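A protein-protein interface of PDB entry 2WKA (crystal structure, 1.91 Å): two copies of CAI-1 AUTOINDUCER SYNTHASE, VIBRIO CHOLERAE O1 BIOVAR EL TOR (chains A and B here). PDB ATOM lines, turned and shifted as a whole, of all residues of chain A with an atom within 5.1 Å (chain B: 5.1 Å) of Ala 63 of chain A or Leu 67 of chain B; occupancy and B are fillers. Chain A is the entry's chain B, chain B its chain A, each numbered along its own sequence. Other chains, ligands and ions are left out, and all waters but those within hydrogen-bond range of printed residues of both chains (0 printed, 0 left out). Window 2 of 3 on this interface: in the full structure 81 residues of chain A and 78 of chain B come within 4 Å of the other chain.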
ATOM      1  N   ILE A  58      25.727 -32.519  20.346  1.00  0.00           N
ATOM      2  CA  ILE A  58      26.307 -31.894  21.534  1.00  0.00           C
ATOM      3  C   ILE A  58      26.128 -30.380  21.464  1.00  0.00           C
ATOM      4  O   ILE A  58      25.712 -29.739  22.435  1.00  0.00           O
ATOM      5  CB  ILE A  58      27.810 -32.227  21.668  1.00  0.00           C
ATOM      6  CG1 ILE A  58      28.008 -33.722  21.909  1.00  0.00           C
ATOM      7  CG2 ILE A  58      28.432 -31.448  22.803  1.00  0.00           C
ATOM      8  CD1 ILE A  58      29.462 -34.103  22.184  1.00  0.00           C
ATOM      9  N   LYS A  59      26.452 -29.809  20.311  1.00  0.00           N
ATOM     10  CA  LYS A  59      26.324 -28.372  20.115  1.00  0.00           C
ATOM     11  C   LYS A  59      24.874 -27.923  20.304  1.00  0.00           C
ATOM     12  O   LYS A  59      24.613 -26.870  20.875  1.00  0.00           O
ATOM     13  CB  LYS A  59      26.848 -27.970  18.734  1.00  0.00           C
ATOM     14  CG  LYS A  59      28.311 -28.339  18.508  1.00  0.00           C
ATOM     15  CD  LYS A  59      28.961 -27.487  17.429  1.00  0.00           C
ATOM     16  CE  LYS A  59      28.182 -27.536  16.119  1.00  0.00           C
ATOM     17  NZ  LYS A  59      28.909 -26.830  15.012  1.00  0.00           N
ATOM     18  N   ALA A  60      23.929 -28.740  19.849  1.00  0.00           N
ATOM     19  CA  ALA A  60      22.510 -28.400  19.975  1.00  0.00           C
ATOM     20  C   ALA A  60      22.050 -28.425  21.430  1.00  0.00           C
ATOM     21  O   ALA A  60      21.370 -27.500  21.892  1.00  0.00           O
ATOM     22  CB  ALA A  60      21.649 -29.330  19.114  1.00  0.00           C
ATOM     23  N   ARG A  61      22.429 -29.475  22.156  1.00  0.00           N
ATOM     24  CA  ARG A  61      22.095 -29.589  23.576  1.00  0.00           C
ATOM     25  C   ARG A  61      22.617 -28.402  24.386  1.00  0.00           C
ATOM     26  O   ARG A  61      21.900 -27.851  25.216  1.00  0.00           O
ATOM     27  CB  ARG A  61      22.647 -30.897  24.157  1.00  0.00           C
ATOM     28  CG  ARG A  61      22.362 -31.098  25.639  1.00  0.00           C
ATOM     29  CD  ARG A  61      20.972 -31.696  25.853  1.00  0.00           C
ATOM     30  NE  ARG A  61      20.551 -31.658  27.253  1.00  0.00           N
ATOM     31  CZ  ARG A  61      20.664 -32.677  28.103  1.00  0.00           C
ATOM     32  NH1 ARG A  61      21.190 -33.829  27.709  1.00  0.00           N
ATOM     33  NH2 ARG A  61      20.246 -32.546  29.355  1.00  0.00           N
ATOM     34  N   LEU A  62      23.870 -28.018  24.151  1.00  0.00           N
ATOM     35  CA  LEU A  62      24.458 -26.846  24.806  1.00  0.00           C
ATOM     36  C   LEU A  62      23.774 -25.535  24.413  1.00  0.00           C
ATOM     37  O   LEU A  62      23.401 -24.743  25.272  1.00  0.00           O
ATOM     38  CB  LEU A  62      25.943 -26.732  24.466  1.00  0.00           C
ATOM     39  CG  LEU A  62      26.989 -27.410  25.342  1.00  0.00           C
ATOM     40  CD1 LEU A  62      28.357 -27.129  24.741  1.00  0.00           C
ATOM     41  CD2 LEU A  62      26.930 -26.918  26.789  1.00  0.00           C
ATOM     42  N   ALA A  63      23.640 -25.289  23.115  1.00  0.00           N
ATOM     43  CA  ALA A  63      22.976 -24.070  22.657  1.00  0.00           C
ATOM     44  C   ALA A  63      21.608 -23.952  23.306  1.00  0.00           C
ATOM     45  O   ALA A  63      21.273 -22.924  23.895  1.00  0.00           O
ATOM     46  CB  ALA A  63      22.852 -24.062  21.141  1.00  0.00           C
ATOM     47  N   LYS A  64      20.827 -25.024  23.206  1.00  0.00           N
ATOM     48  CA  LYS A  64      19.500 -25.088  23.800  1.00  0.00           C
ATOM     49  C   LYS A  64      19.547 -24.722  25.266  1.00  0.00           C
ATOM     50  O   LYS A  64      18.870 -23.790  25.711  1.00  0.00           O
ATOM     51  CB  LYS A  64      18.938 -26.505  23.681  1.00  0.00           C
ATOM     52  CG  LYS A  64      17.438 -26.575  23.497  1.00  0.00           C
ATOM     53  CD  LYS A  64      16.950 -28.027  23.495  1.00  0.00           C
ATOM     54  CE  LYS A  64      18.085 -28.990  23.170  1.00  0.00           C
ATOM     55  NZ  LYS A  64      17.579 -30.335  22.766  1.00  0.00           N
ATOM     56  N   SER A  65      20.333 -25.483  26.020  1.00  0.00           N
ATOM     57  CA  SER A  65      20.425 -25.280  27.460  1.00  0.00           C
ATOM     58  C   SER A  65      20.912 -23.878  27.814  1.00  0.00           C
ATOM     59  O   SER A  65      20.467 -23.308  28.798  1.00  0.00           O
ATOM     60  CB  SER A  65      21.332 -26.334  28.111  1.00  0.00           C
ATOM     61  OG  SER A  65      20.714 -27.610  28.078  1.00  0.00           O
ATOM     62  N   LEU A  66      21.831 -23.319  27.037  1.00  0.00           N
ATOM     63  CA  LEU A  66      22.306 -21.987  27.387  1.00  0.00           C
ATOM     64  C   LEU A  66      21.283 -20.923  27.014  1.00  0.00           C
ATOM     65  O   LEU A  66      20.845 -20.163  27.881  1.00  0.00           O
ATOM     66  CB  LEU A  66      23.696 -21.695  26.831  1.00  0.00           C
ATOM     67  CG  LEU A  66      23.942 -21.286  25.389  1.00  0.00           C
ATOM     68  CD1 LEU A  66      23.841 -19.781  25.267  1.00  0.00           C
ATOM     69  CD2 LEU A  66      25.334 -21.754  25.014  1.00  0.00           C
ATOM     70  N   LEU A  67      20.908 -20.866  25.734  1.00  0.00           N
ATOM     71  CA  LEU A  67      19.745 -20.080  25.344  1.00  0.00           C
ATOM     72  C   LEU A  67      18.810 -20.434  26.463  1.00  0.00           C
ATOM     73  O   LEU A  67      18.957 -21.494  27.060  1.00  0.00           O
ATOM     74  CB  LEU A  67      19.172 -20.556  24.009  1.00  0.00           C
ATOM     75  CG  LEU A  67      19.510 -19.770  22.741  1.00  0.00           C
ATOM     76  CD1 LEU A  67      20.680 -18.816  22.947  1.00  0.00           C
ATOM     77  CD2 LEU A  67      19.764 -20.708  21.567  1.00  0.00           C
ATOM     78  N   LEU B  62      26.674 -16.336  22.327  1.00  0.00           N
ATOM     79  CA  LEU B  62      27.313 -17.583  22.748  1.00  0.00           C
ATOM     80  C   LEU B  62      26.778 -18.766  21.943  1.00  0.00           C
ATOM     81  O   LEU B  62      27.545 -19.558  21.401  1.00  0.00           O
ATOM     82  CB  LEU B  62      27.073 -17.859  24.239  1.00  0.00           C
ATOM     83  CG  LEU B  62      28.193 -17.687  25.267  1.00  0.00           C
ATOM     84  CD1 LEU B  62      27.691 -18.137  26.631  1.00  0.00           C
ATOM     85  CD2 LEU B  62      29.444 -18.475  24.867  1.00  0.00           C
ATOM     86  N   ALA B  63      25.455 -18.895  21.902  1.00  0.00           N
ATOM     87  CA  ALA B  63      24.820 -20.009  21.185  1.00  0.00           C
ATOM     88  C   ALA B  63      25.225 -19.986  19.724  1.00  0.00           C
ATOM     89  O   ALA B  63      25.540 -21.023  19.136  1.00  0.00           O
ATOM     90  CB  ALA B  63      23.311 -19.940  21.315  1.00  0.00           C
ATOM     91  N   LYS B  64      25.215 -18.795  19.137  1.00  0.00           N
ATOM     92  CA  LYS B  64      25.616 -18.635  17.745  1.00  0.00           C
ATOM     93  C   LYS B  64      27.022 -19.172  17.471  1.00  0.00           C
ATOM     94  O   LYS B  64      27.194 -20.071  16.654  1.00  0.00           O
ATOM     95  CB  LYS B  64      25.521 -17.173  17.319  1.00  0.00           C
ATOM     96  CG  LYS B  64      25.704 -16.972  15.825  1.00  0.00           C
ATOM     97  CD  LYS B  64      25.371 -15.551  15.414  1.00  0.00           C
ATOM     98  CE  LYS B  64      26.538 -14.626  15.689  1.00  0.00           C
ATOM     99  NZ  LYS B  64      27.751 -15.165  15.008  1.00  0.00           N
ATOM    100  N   SER B  65      28.029 -18.626  18.147  1.00  0.00           N
ATOM    101  CA  SER B  65      29.400 -19.078  17.903  1.00  0.00           C
ATOM    102  C   SER B  65      29.598 -20.544  18.291  1.00  0.00           C
ATOM    103  O   SER B  65      30.418 -21.236  17.704  1.00  0.00           O
ATOM    104  CB  SER B  65      30.424 -18.183  18.608  1.00  0.00           C
ATOM    105  OG  SER B  65      29.945 -17.793  19.874  1.00  0.00           O
ATOM    106  N   LEU B  66      28.846 -21.012  19.275  1.00  0.00           N
ATOM    107  CA  LEU B  66      28.903 -22.418  19.651  1.00  0.00           C
ATOM    108  C   LEU B  66      28.387 -23.306  18.513  1.00  0.00           C
ATOM    109  O   LEU B  66      28.926 -24.383  18.253  1.00  0.00           O
ATOM    110  CB  LEU B  66      28.077 -22.671  20.905  1.00  0.00           C
ATOM    111  CG  LEU B  66      27.894 -24.163  21.138  1.00  0.00           C
ATOM    112  CD1 LEU B  66      26.595 -24.415  21.885  1.00  0.00           C
ATOM    113  CD2 LEU B  66      27.901 -24.861  19.782  1.00  0.00           C
ATOM    114  N   LEU B  67      27.332 -22.848  17.844  1.00  0.00           N
ATOM    115  CA  LEU B  67      26.733 -23.599  16.743  1.00  0.00           C
ATOM    116  C   LEU B  67      27.602 -23.556  15.495  1.00  0.00           C
ATOM    117  O   LEU B  67      27.528 -24.445  14.652  1.00  0.00           O
ATOM    118  CB  LEU B  67      25.330 -23.071  16.428  1.00  0.00           C
ATOM    119  CG  LEU B  67      24.249 -23.415  17.449  1.00  0.00           C
ATOM    120  CD1 LEU B  67      22.932 -22.738  17.084  1.00  0.00           C
ATOM    121  CD2 LEU B  67      24.063 -24.921  17.566  1.00  0.00           C
ATOM    122  N   GLU B  68      28.434 -22.529  15.379  1.00  0.00           N
ATOM    123  CA  GLU B  68      29.316 -22.410  14.225  1.00  0.00           C
ATOM    124  C   GLU B  68      30.318 -23.553  14.117  1.00  0.00           C
ATOM    125  O   GLU B  68      31.002 -23.702  13.103  1.00  0.00           O
ATOM    126  CB  GLU B  68      30.040 -21.064  14.221  1.00  0.00           C
ATOM    127  CG  GLU B  68      29.524 -20.127  13.141  1.00  0.00           C
ATOM    128  CD  GLU B  68      29.573 -18.673  13.540  1.00  0.00           C
ATOM    129  OE1 GLU B  68      30.342 -18.329  14.457  1.00  0.00           O
ATOM    130  OE2 GLU B  68      28.837 -17.871  12.932  1.00  0.00           O
ATOM    131  N   GLU B  69      30.431 -24.364  15.158  1.00  0.00           N
ATOM    132  CA  GLU B  69      31.326 -25.493  15.037  1.00  0.00           C
ATOM    133  C   GLU B  69      32.523 -25.522  15.960  1.00  0.00           C
ATOM    134  O   GLU B  69      32.604 -24.825  16.985  1.00  0.00           O
ATOM    135  CB  GLU B  69      31.879 -25.551  13.611  1.00  0.00           C
ATOM    136  CG  GLU B  69      33.408 -25.598  13.577  1.00  0.00           C
ATOM    137  CD  GLU B  69      34.039 -24.230  13.759  1.00  0.00           C
ATOM    138  OE1 GLU B  69      33.310 -23.283  14.108  1.00  0.00           O
ATOM    139  OE2 GLU B  69      35.262 -24.090  13.536  1.00  0.00           O
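Leu 62 of chain A touches Leu 66 of chain B, and with the chains exchanged Leu 66 of chain A touches Leu 62 of chain B. Ala 63 of chain A touches Leu 66 of chain B, and with the chains exchanged Leu 66 of chain A touches Ala 63 of chain B. Ala 63 of chain A touches Leu 67 of chain B, and with the chains exchanged Leu 67 of chain A touches Ala 63 of chain B.
The backbone carbonyl oxygen (O) of Leu 67 of chain B sits at hydrogen-bond distance from the side-chain amino group (NZ) of Lys 59 of chain A, at 2.8 Å. NZ of Lys 59 of chain A sits close to N of Glu 69 of chain B (2.9 Å).
The backbone carbonyl oxygen of Leu 62 of chain B is in hydrogen-bond range of the side-chain hydroxyl of Ser 65 of chain B, 3.3 Å away. The side-chain amino group (NZ) of Lys 64 of chain B lies within salt-bridge range of the side-chain carboxylate (OE2) of Glu 68 of chain B (3.6 Å).
Printed residues of chain B that touch a printed residue of chain A: Leu 62, Ala 63, Leu 66, Leu 67, Glu 68 and Glu 69. Hydrophobic or aromatic side chains of chain B that line the printed part of chain A: Leu 62, Ala 63, Leu 66 and Leu 67. Of the 10 printed residues of chain A, 5 touch a printed residue of chain B.
Of chain B, only Leu 66 (3.3 Å) and Leu 67 (3.9 Å) come within 4 Å of Ala 63 of chain A. Printed residues of chain A within 4 Å of Glu 68 of chain B: Lys 59. Of the printed residues of chain A, Leu 66 of chain B touches Lys 59, Leu 62 and Ala 63. Of the printed residues of chain A, Leu 62 of chain B touches Leu 66. The nearest residue of chain A that does not touch Leu 67 of chain B is Ala 60 of chain A (4.5 Å).
Lys 59 of chain A touches Leu 66 of chain B. NZ of Lys 59 of chain A touches C of Glu 68 of chain B, 3.7 Å away. Leu 62 of chain A touches Leu 66 of chain B. Ala 63 of chain A touches Leu 66 of chain B. CB of Ala 63 of chain A touches CD2 of Leu 67 of chain B (3.9 Å). Leu 62 of chain B touches Leu 66 of chain A. Ala 63 of chain B touches Leu 66 of chain A. CD1 of Leu 67 of chain A touches CB of Ala 63 of chain B, at 3.3 Å.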
